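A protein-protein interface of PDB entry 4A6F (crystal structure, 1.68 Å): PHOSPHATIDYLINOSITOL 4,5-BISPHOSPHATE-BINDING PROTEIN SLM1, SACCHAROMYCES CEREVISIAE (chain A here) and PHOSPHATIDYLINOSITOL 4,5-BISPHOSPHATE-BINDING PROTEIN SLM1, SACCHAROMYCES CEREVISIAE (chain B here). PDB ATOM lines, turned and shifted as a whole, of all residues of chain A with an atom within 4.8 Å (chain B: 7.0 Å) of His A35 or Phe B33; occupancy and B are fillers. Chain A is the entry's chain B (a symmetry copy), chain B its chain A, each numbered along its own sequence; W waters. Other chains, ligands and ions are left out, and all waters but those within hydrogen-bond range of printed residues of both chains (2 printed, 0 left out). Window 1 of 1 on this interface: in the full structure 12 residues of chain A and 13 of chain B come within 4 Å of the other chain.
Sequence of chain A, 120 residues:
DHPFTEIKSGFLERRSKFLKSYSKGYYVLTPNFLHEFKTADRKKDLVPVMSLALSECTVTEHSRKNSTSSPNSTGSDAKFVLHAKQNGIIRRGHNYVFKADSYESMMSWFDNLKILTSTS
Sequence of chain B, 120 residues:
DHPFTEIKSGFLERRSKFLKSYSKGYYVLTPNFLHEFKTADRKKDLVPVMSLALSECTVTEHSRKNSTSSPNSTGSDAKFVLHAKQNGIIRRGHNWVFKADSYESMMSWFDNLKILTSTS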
ATOM      1  N   TYR A  26      15.589  15.388 -10.827  1.00  0.00           N
ATOM      2  CA  TYR A  26      14.978  14.380  -9.987  1.00  0.00           C
ATOM      3  C   TYR A  26      15.146  14.845  -8.556  1.00  0.00           C
ATOM      4  O   TYR A  26      16.268  15.076  -8.105  1.00  0.00           O
ATOM      5  CB  TYR A  26      15.654  13.021 -10.187  1.00  0.00           C
ATOM      6  CG  TYR A  26      14.963  11.917  -9.439  1.00  0.00           C
ATOM      7  CD1 TYR A  26      13.784  11.361  -9.928  1.00  0.00           C
ATOM      8  CD2 TYR A  26      15.458  11.453  -8.232  1.00  0.00           C
ATOM      9  CE1 TYR A  26      13.129  10.359  -9.241  1.00  0.00           C
ATOM     10  CE2 TYR A  26      14.811  10.446  -7.535  1.00  0.00           C
ATOM     11  CZ  TYR A  26      13.647   9.906  -8.052  1.00  0.00           C
ATOM     12  OH  TYR A  26      13.002   8.907  -7.365  1.00  0.00           O
ATOM     13  N   TYR A  27      14.038  15.000  -7.846  1.00  0.00           N
ATOM     14  CA  TYR A  27      14.084  15.583  -6.516  1.00  0.00           C
ATOM     15  C   TYR A  27      13.752  14.558  -5.457  1.00  0.00           C
ATOM     16  O   TYR A  27      12.907  13.687  -5.658  1.00  0.00           O
ATOM     17  CB  TYR A  27      13.094  16.756  -6.434  1.00  0.00           C
ATOM     18  CG  TYR A  27      13.578  17.975  -7.183  1.00  0.00           C
ATOM     19  CD1 TYR A  27      13.462  18.052  -8.572  1.00  0.00           C
ATOM     20  CD2 TYR A  27      14.174  19.032  -6.512  1.00  0.00           C
ATOM     21  CE1 TYR A  27      13.914  19.166  -9.265  1.00  0.00           C
ATOM     22  CE2 TYR A  27      14.637  20.142  -7.192  1.00  0.00           C
ATOM     23  CZ  TYR A  27      14.500  20.205  -8.568  1.00  0.00           C
ATOM     24  OH  TYR A  27      14.962  21.306  -9.237  1.00  0.00           O
ATOM     25  N   VAL A  28      14.426  14.688  -4.320  1.00  0.00           N
ATOM     26  CA  VAL A  28      14.163  13.859  -3.150  1.00  0.00           C
ATOM     27  C   VAL A  28      13.896  14.764  -1.953  1.00  0.00           C
ATOM     28  O   VAL A  28      14.735  15.575  -1.576  1.00  0.00           O
ATOM     29  CB  VAL A  28      15.335  12.890  -2.851  1.00  0.00           C
ATOM     30  CG1 VAL A  28      15.050  12.113  -1.570  1.00  0.00           C
ATOM     31  CG2 VAL A  28      15.532  11.933  -4.017  1.00  0.00           C
ATOM     32  N   THR A  30      13.317  15.000   1.983  1.00  0.00           N
ATOM     33  CA  THR A  30      13.554  14.308   3.232  1.00  0.00           C
ATOM     34  C   THR A  30      12.961  15.169   4.333  1.00  0.00           C
ATOM     35  O   THR A  30      12.486  16.278   4.062  1.00  0.00           O
ATOM     36  CB  THR A  30      15.065  14.082   3.448  1.00  0.00           C
ATOM     37  OG1 THR A  30      15.711  15.338   3.672  1.00  0.00           O
ATOM     38  CG2 THR A  30      15.694  13.419   2.218  1.00  0.00           C
ATOM     39  N   PHE A  33      15.541  18.293   3.957  1.00  0.00           N
ATOM     40  CA  PHE A  33      16.004  18.946   2.736  1.00  0.00           C
ATOM     41  C   PHE A  33      15.123  18.634   1.538  1.00  0.00           C
ATOM     42  O   PHE A  33      14.482  17.583   1.479  1.00  0.00           O
ATOM     43  CB  PHE A  33      17.398  18.432   2.362  1.00  0.00           C
ATOM     44  CG  PHE A  33      18.499  18.962   3.216  1.00  0.00           C
ATOM     45  CD1 PHE A  33      18.955  20.261   3.046  1.00  0.00           C
ATOM     46  CD2 PHE A  33      19.112  18.150   4.158  1.00  0.00           C
ATOM     47  CE1 PHE A  33      19.989  20.750   3.825  1.00  0.00           C
ATOM     48  CE2 PHE A  33      20.151  18.636   4.933  1.00  0.00           C
ATOM     49  CZ  PHE A  33      20.585  19.931   4.758  1.00  0.00           C
ATOM     50  N   LEU A  34      15.109  19.557   0.585  1.00  0.00           N
ATOM     51  CA  LEU A  34      14.705  19.222  -0.779  1.00  0.00           C
ATOM     52  C   LEU A  34      15.996  19.114  -1.574  1.00  0.00           C
ATOM     53  O   LEU A  34      16.668  20.120  -1.818  1.00  0.00           O
ATOM     54  CB  LEU A  34      13.786  20.295  -1.375  1.00  0.00           C
ATOM     55  CG  LEU A  34      13.295  19.995  -2.795  1.00  0.00           C
ATOM     56  CD1 LEU A  34      12.463  18.716  -2.828  1.00  0.00           C
ATOM     57  CD2 LEU A  34      12.495  21.177  -3.362  1.00  0.00           C
ATOM     58  N   HIS A  35      16.374  17.886  -1.930  1.00  0.00           N
ATOM     59  CA  HIS A  35      17.593  17.648  -2.694  1.00  0.00           C
ATOM     60  C   HIS A  35      17.283  17.547  -4.187  1.00  0.00           C
ATOM     61  O   HIS A  35      16.305  16.910  -4.580  1.00  0.00           O
ATOM     62  CB  HIS A  35      18.253  16.316  -2.305  1.00  0.00           C
ATOM     63  CG  HIS A  35      18.674  16.210  -0.867  1.00  0.00           C
ATOM     64  ND1 HIS A  35      19.714  16.937  -0.330  1.00  0.00           N
ATOM     65  CD2 HIS A  35      18.233  15.397   0.123  1.00  0.00           C
ATOM     66  CE1 HIS A  35      19.874  16.604   0.939  1.00  0.00           C
ATOM     67  NE2 HIS A  35      18.993  15.665   1.238  1.00  0.00           N
ATOM     68  N   GLU A  36      18.140  18.141  -5.012  1.00  0.00           N
ATOM     69  CA  GLU A  36      18.051  17.949  -6.459  1.00  0.00           C
ATOM     70  C   GLU A  36      19.157  17.027  -6.951  1.00  0.00           C
ATOM     71  O   GLU A  36      20.326  17.211  -6.600  1.00  0.00           O
ATOM     72  CB  GLU A  36      18.184  19.284  -7.192  1.00  0.00           C
ATOM     73  CG  GLU A  36      18.067  19.149  -8.715  1.00  0.00           C
ATOM     74  CD  GLU A  36      18.489  20.415  -9.457  1.00  0.00           C
ATOM     75  OE1 GLU A  36      18.847  21.409  -8.793  1.00  0.00           O
ATOM     76  OE2 GLU A  36      18.456  20.415 -10.704  1.00  0.00           O
ATOM     77  N   PHE A  37      18.786  16.042  -7.772  1.00  0.00           N
ATOM     78  CA  PHE A  37      19.761  15.193  -8.464  1.00  0.00           C
ATOM     79  C   PHE A  37      19.551  15.295  -9.980  1.00  0.00           C
ATOM     80  O   PHE A  37      18.467  15.625 -10.453  1.00  0.00           O
ATOM     81  CB  PHE A  37      19.638  13.719  -8.046  1.00  0.00           C
ATOM     82  CG  PHE A  37      19.843  13.477  -6.575  1.00  0.00           C
ATOM     83  CD1 PHE A  37      18.788  13.573  -5.694  1.00  0.00           C
ATOM     84  CD2 PHE A  37      21.091  13.108  -6.088  1.00  0.00           C
ATOM     85  CE1 PHE A  37      18.981  13.346  -4.333  1.00  0.00           C
ATOM     86  CE2 PHE A  37      21.286  12.868  -4.742  1.00  0.00           C
ATOM     87  CZ  PHE A  37      20.237  12.982  -3.864  1.00  0.00           C
ATOM     88  N   LEU A  46      24.665  10.082  -6.602  1.00  0.00           N
ATOM     89  CA  LEU A  46      24.479  10.207  -5.160  1.00  0.00           C
ATOM     90  C   LEU A  46      24.840  11.560  -4.556  1.00  0.00           C
ATOM     91  O   LEU A  46      24.661  11.762  -3.355  1.00  0.00           O
ATOM     92  CB  LEU A  46      25.240   9.092  -4.436  1.00  0.00           C
ATOM     93  CG  LEU A  46      24.595   7.722  -4.627  1.00  0.00           C
ATOM     94  CD1 LEU A  46      25.154   6.744  -3.636  1.00  0.00           C
ATOM     95  CD2 LEU A  46      23.092   7.854  -4.439  1.00  0.00           C
ATOM     96  N   PRO A  48      23.900  15.397  -4.387  1.00  0.00           N
ATOM     97  CA  PRO A  48      22.899  16.376  -4.821  1.00  0.00           C
ATOM     98  C   PRO A  48      23.568  17.515  -5.573  1.00  0.00           C
ATOM     99  O   PRO A  48      24.648  17.955  -5.159  1.00  0.00           O
ATOM    100  CB  PRO A  48      22.342  16.921  -3.502  1.00  0.00           C
ATOM    101  CG  PRO A  48      22.653  15.879  -2.481  1.00  0.00           C
ATOM    102  CD  PRO A  48      23.936  15.234  -2.924  1.00  0.00           C
ATOM    103  N   MET A  50      22.099  20.276  -5.569  1.00  0.00           N
ATOM    104  CA  MET A  50      21.694  21.325  -4.643  1.00  0.00           C
ATOM    105  C   MET A  50      20.851  20.711  -3.539  1.00  0.00           C
ATOM    106  O   MET A  50      20.074  19.785  -3.788  1.00  0.00           O
ATOM    107  CB  MET A  50      20.880  22.391  -5.385  1.00  0.00           C
ATOM    108  CG  MET A  50      19.996  23.249  -4.495  1.00  0.00           C
ATOM    109  SD  MET A  50      18.697  24.084  -5.429  1.00  0.00           S
ATOM    110  CE  MET A  50      17.562  22.731  -5.746  1.00  0.00           C
ATOM    111  N   SER A  51      21.021  21.208  -2.318  1.00  0.00           N
ATOM    112  CA  SER A  51      20.173  20.812  -1.201  1.00  0.00           C
ATOM    113  C   SER A  51      19.590  22.066  -0.551  1.00  0.00           C
ATOM    114  O   SER A  51      20.333  22.920  -0.060  1.00  0.00           O
ATOM    115  CB  SER A  51      20.975  20.028  -0.151  1.00  0.00           C
ATOM    116  OG  SER A  51      21.572  18.866  -0.716  1.00  0.00           O
ATOM    117  N   VAL B  28      27.222  16.470  10.623  1.00  0.00           N
ATOM    118  CA  VAL B  28      25.897  16.057  11.031  1.00  0.00           C
ATOM    119  C   VAL B  28      25.569  14.771  10.308  1.00  0.00           C
ATOM    120  O   VAL B  28      25.570  14.716   9.078  1.00  0.00           O
ATOM    121  CB  VAL B  28      24.830  17.116  10.679  1.00  0.00           C
ATOM    122  CG1 VAL B  28      23.462  16.620  11.064  1.00  0.00           C
ATOM    123  CG2 VAL B  28      25.156  18.445  11.387  1.00  0.00           C
ATOM    124  N   LEU B  29      25.294  13.739  11.089  1.00  0.00           N
ATOM    125  CA  LEU B  29      24.921  12.437  10.554  1.00  0.00           C
ATOM    126  C   LEU B  29      23.400  12.265  10.545  1.00  0.00           C
ATOM    127  O   LEU B  29      22.753  12.383  11.579  1.00  0.00           O
ATOM    128  CB  LEU B  29      25.565  11.342  11.407  1.00  0.00           C
ATOM    129  CG  LEU B  29      25.291   9.894  11.010  1.00  0.00           C
ATOM    130  CD1 LEU B  29      25.821   9.575   9.600  1.00  0.00           C
ATOM    131  CD2 LEU B  29      25.932   8.970  12.036  1.00  0.00           C
ATOM    132  N   THR B  30      22.832  11.980   9.375  1.00  0.00           N
ATOM    133  CA  THR B  30      21.404  11.673   9.263  1.00  0.00           C
ATOM    134  C   THR B  30      21.281  10.237   8.760  1.00  0.00           C
ATOM    135  O   THR B  30      22.285   9.593   8.513  1.00  0.00           O
ATOM    136  CB  THR B  30      20.691  12.612   8.277  1.00  0.00           C
ATOM    137  OG1 THR B  30      21.142  12.313   6.953  1.00  0.00           O
ATOM    138  CG2 THR B  30      20.988  14.048   8.613  1.00  0.00           C
ATOM    139  N   PRO B  31      20.047   9.723   8.607  1.00  0.00           N
ATOM    140  CA  PRO B  31      19.961   8.365   8.055  1.00  0.00           C
ATOM    141  C   PRO B  31      20.426   8.258   6.605  1.00  0.00           C
ATOM    142  O   PRO B  31      20.672   7.151   6.137  1.00  0.00           O
ATOM    143  CB  PRO B  31      18.468   8.039   8.159  1.00  0.00           C
ATOM    144  CG  PRO B  31      17.973   8.890   9.285  1.00  0.00           C
ATOM    145  CD  PRO B  31      18.757  10.177   9.162  1.00  0.00           C
ATOM    146  N   ASN B  32      20.574   9.386   5.917  1.00  0.00           N
ATOM    147  CA  ASN B  32      20.928   9.358   4.502  1.00  0.00           C
ATOM    148  C   ASN B  32      22.351   9.820   4.194  1.00  0.00           C
ATOM    149  O   ASN B  32      22.971   9.306   3.275  1.00  0.00           O
ATOM    150  CB  ASN B  32      19.943  10.193   3.691  1.00  0.00           C
ATOM    151  CG  ASN B  32      18.573   9.566   3.634  1.00  0.00           C
ATOM    152  OD1 ASN B  32      18.436   8.348   3.697  1.00  0.00           O
ATOM    153  ND2 ASN B  32      17.552  10.393   3.501  1.00  0.00           N
ATOM    154  N   PHE B  33      22.849  10.792   4.954  1.00  0.00           N
ATOM    155  CA  PHE B  33      24.129  11.439   4.636  1.00  0.00           C
ATOM    156  C   PHE B  33      24.985  11.704   5.863  1.00  0.00           C
ATOM    157  O   PHE B  33      24.480  11.836   6.982  1.00  0.00           O
ATOM    158  CB  PHE B  33      23.900  12.815   4.007  1.00  0.00           C
ATOM    159  CG  PHE B  33      23.318  12.782   2.626  1.00  0.00           C
ATOM    160  CD1 PHE B  33      24.118  12.535   1.526  1.00  0.00           C
ATOM    161  CD2 PHE B  33      21.975  13.041   2.430  1.00  0.00           C
ATOM    162  CE1 PHE B  33      23.577  12.520   0.249  1.00  0.00           C
ATOM    163  CE2 PHE B  33      21.425  13.030   1.156  1.00  0.00           C
ATOM    164  CZ  PHE B  33      22.232  12.774   0.065  1.00  0.00           C
ATOM    165  N   LEU B  34      26.288  11.813   5.629  1.00  0.00           N
ATOM    166  CA  LEU B  34      27.167  12.513   6.553  1.00  0.00           C
ATOM    167  C   LEU B  34      27.403  13.872   5.917  1.00  0.00           C
ATOM    168  O   LEU B  34      28.027  13.962   4.857  1.00  0.00           O
ATOM    169  CB  LEU B  34      28.493  11.765   6.733  1.00  0.00           C
ATOM    170  CG  LEU B  34      29.505  12.464   7.663  1.00  0.00           C
ATOM    171  CD1 LEU B  34      29.043  12.528   9.110  1.00  0.00           C
ATOM    172  CD2 LEU B  34      30.845  11.712   7.601  1.00  0.00           C
ATOM    173  N   HIS B  35      26.862  14.930   6.521  1.00  0.00           N
ATOM    174  CA  HIS B  35      27.003  16.278   5.971  1.00  0.00           C
ATOM    175  C   HIS B  35      28.126  16.999   6.686  1.00  0.00           C
ATOM    176  O   HIS B  35      28.241  16.893   7.906  1.00  0.00           O
ATOM    177  CB  HIS B  35      25.740  17.109   6.226  1.00  0.00           C
ATOM    178  CG  HIS B  35      24.505  16.581   5.583  1.00  0.00           C
ATOM    179  ND1 HIS B  35      24.284  16.640   4.223  1.00  0.00           N
ATOM    180  CD2 HIS B  35      23.388  16.034   6.122  1.00  0.00           C
ATOM    181  CE1 HIS B  35      23.104  16.115   3.948  1.00  0.00           C
ATOM    182  NE2 HIS B  35      22.532  15.755   5.087  1.00  0.00           N
ATOM    183  N   PRO B  48      25.115  22.431   3.316  1.00  0.00           N
ATOM    184  CA  PRO B  48      26.312  21.616   3.545  1.00  0.00           C
ATOM    185  C   PRO B  48      27.437  21.978   2.582  1.00  0.00           C
ATOM    186  O   PRO B  48      27.189  22.240   1.405  1.00  0.00           O
ATOM    187  CB  PRO B  48      25.838  20.183   3.260  1.00  0.00           C
ATOM    188  CG  PRO B  48      24.355  20.221   3.407  1.00  0.00           C
ATOM    189  CD  PRO B  48      23.925  21.614   3.023  1.00  0.00           C
ATOM    190  N   MET B  50      29.599  19.646   1.982  1.00  0.00           N
ATOM    191  CA  MET B  50      29.744  18.333   1.383  1.00  0.00           C
ATOM    192  C   MET B  50      28.667  17.427   1.981  1.00  0.00           C
ATOM    193  O   MET B  50      28.374  17.508   3.178  1.00  0.00           O
ATOM    194  CB  MET B  50      31.138  17.777   1.715  1.00  0.00           C
ATOM    195  CG  MET B  50      31.325  16.305   1.398  1.00  0.00           C
ATOM    196  SD  MET B  50      32.964  15.719   1.878  1.00  0.00           S
ATOM    197  CE  MET B  50      32.791  15.647   3.666  1.00  0.00           C
ATOM    198  N   SER B  51      28.065  16.584   1.153  1.00  0.00           N
ATOM    199  CA  SER B  51      27.123  15.583   1.649  1.00  0.00           C
ATOM    200  C   SER B  51      27.516  14.227   1.100  1.00  0.00           C
ATOM    201  O   SER B  51      27.387  13.987  -0.107  1.00  0.00           O
ATOM    202  CB  SER B  51      25.691  15.904   1.209  1.00  0.00           C
ATOM    203  OG  SER B  51      25.262  17.150   1.729  1.00  0.00           O
ATOM    204  N   LEU B  52      27.993  13.360   1.990  1.00  0.00           N
ATOM    205  CA  LEU B  52      28.455  12.021   1.637  1.00  0.00           C
ATOM    206  C   LEU B  52      27.319  11.025   1.811  1.00  0.00           C
ATOM    207  O   LEU B  52      26.888  10.743   2.942  1.00  0.00           O
ATOM    208  CB  LEU B  52      29.635  11.597   2.519  1.00  0.00           C
ATOM    209  CG  LEU B  52      31.002  12.285   2.384  1.00  0.00           C
ATOM    210  CD1 LEU B  52      31.916  11.937   3.561  1.00  0.00           C
ATOM    211  CD2 LEU B  52      31.677  11.924   1.068  1.00  0.00           C
ATOM    212  N   ALA B  53      26.845  10.492   0.691  1.00  0.00           N
ATOM    213  CA  ALA B  53      25.771   9.499   0.693  1.00  0.00           C
ATOM    214  C   ALA B  53      26.175   8.201   1.394  1.00  0.00           C
ATOM    215  O   ALA B  53      27.096   7.510   0.963  1.00  0.00           O
ATOM    216  CB  ALA B  53      25.320   9.221  -0.741  1.00  0.00           C
ATOM    217  N   LEU B  54      25.470   7.859   2.466  1.00  0.00           N
ATOM    218  CA  LEU B  54      25.814   6.704   3.281  1.00  0.00           C
ATOM    219  C   LEU B  54      25.617   5.388   2.521  1.00  0.00           C
ATOM    220  O   LEU B  54      26.256   4.385   2.824  1.00  0.00           O
ATOM    221  CB  LEU B  54      24.992   6.698   4.573  1.00  0.00           C
ATOM    222  CG  LEU B  54      25.207   7.924   5.469  1.00  0.00           C
ATOM    223  CD1 LEU B  54      24.349   7.843   6.736  1.00  0.00           C
ATOM    224  CD2 LEU B  54      26.671   8.066   5.815  1.00  0.00           C
ATOM    225  N   SER B  55      24.728   5.405   1.532  1.00  0.00           N
ATOM    226  CA  SER B  55      24.393   4.180   0.801  1.00  0.00           C
ATOM    227  C   SER B  55      25.593   3.594   0.062  1.00  0.00           C
ATOM    228  O   SER B  55      25.622   2.400  -0.237  1.00  0.00           O
ATOM    229  CB  SER B  55      23.249   4.429  -0.178  1.00  0.00           C
ATOM    230  OG  SER B  55      23.613   5.394  -1.143  1.00  0.00           O
ATOM    231  N   LEU B 113      28.167   5.263  12.280  1.00  0.00           N
ATOM    232  CA  LEU B 113      28.278   5.165  10.834  1.00  0.00           C
ATOM    233  C   LEU B 113      28.102   3.728  10.381  1.00  0.00           C
ATOM    234  O   LEU B 113      27.440   3.467   9.381  1.00  0.00           O
ATOM    235  CB  LEU B 113      29.636   5.701  10.358  1.00  0.00           C
ATOM    236  CG  LEU B 113      29.683   7.228  10.269  1.00  0.00           C
ATOM    237  CD1 LEU B 113      31.128   7.736  10.243  1.00  0.00           C
ATOM    238  CD2 LEU B 113      28.923   7.685   9.031  1.00  0.00           C
ATOM    239  N   LEU B 116      24.603   2.440   9.937  1.00  0.00           N
ATOM    240  CA  LEU B 116      23.883   3.079   8.846  1.00  0.00           C
ATOM    241  C   LEU B 116      24.463   2.719   7.483  1.00  0.00           C
ATOM    242  O   LEU B 116      23.959   3.173   6.450  1.00  0.00           O
ATOM    243  CB  LEU B 116      23.870   4.606   9.026  1.00  0.00           C
ATOM    244  CG  LEU B 116      22.990   5.161  10.152  1.00  0.00           C
ATOM    245  CD1 LEU B 116      23.288   6.644  10.400  1.00  0.00           C
ATOM    246  CD2 LEU B 116      21.508   4.938   9.864  1.00  0.00           C
HETATM  247  O   HOH W   1      24.365  18.697  -0.394  1.00  0.00           O
HETATM  248  O   HOH W   2      27.152  11.979  -1.869  1.00  0.00           O
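ND1 of His B35 lies within hydrogen-bond range of OG of Ser B51. The backbone NH (N) of Phe B33 lies within hydrogen-bond range of the side-chain hydroxyl (OG1) of Thr B30, at 3.0 Å. O of Asn B32 is in hydrogen-bond range of N of Leu B54. O of Val B28 sits at hydrogen-bond distance from N of His B35 (2.9 Å). OG1 of Thr B30 lies close to N of Asn B32 (3.2 Å). A ring nitrogen (ND1) of His A35 sits at hydrogen-bond distance from the side-chain hydroxyl (OG) of Ser A51, at 2.7 Å.
Of chain B, only Phe B33 comes within 4 Å of His A35. Phe B33 touches two residues of chain A. Of the printed residues of chain A, Ala B53 touches Leu A46. Of the printed residues of chain B, Leu A46 touches Phe B33, Ala B53 and Ser B55. Of the printed residues of chain A, Ser B55 touches Leu A46. Printed residues of chain A within 4 Å of Asn B32: Thr A30. Tyr A26 touches none of the printed residues of chain B. Met B50 touches none of the printed residues of chain A.
Water W2 lies within hydrogen-bond range of O of Ser B51 (2.7 Å), O of Leu A46 (2.9 Å) and N of Ala B53 (3.0 Å). Water W1 lies within hydrogen-bond range of the side-chain hydroxyl (OG) of Ser B51 (2.8 Å) and the side-chain hydroxyl (OG) of Ser A51 (2.8 Å).
Printed residues of chain B that touch a printed residue of chain A: Asn B32, Phe B33, His B35, Ala B53 and Ser B55. Hydrophobic or aromatic side chains of chain B that line the printed part of chain A: Phe B33, His B35 and Ala B53. Hydrophobic or aromatic side chains of chain A that line the printed part of chain B: Phe A33, His A35 and Leu A46. Among the printed residues, no Asp or Glu carboxylate lies within 4 Å of a Lys or Arg side-chain nitrogen of the other chain.
Among the printed residues, pairs that only touch across the chains: Thr A30 with Asn B32, Phe A33 with His B35, His A35 with Phe B33, Leu A46 with Phe B33, Leu A46 with Ala B53 and Leu A46 with Ser B55.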
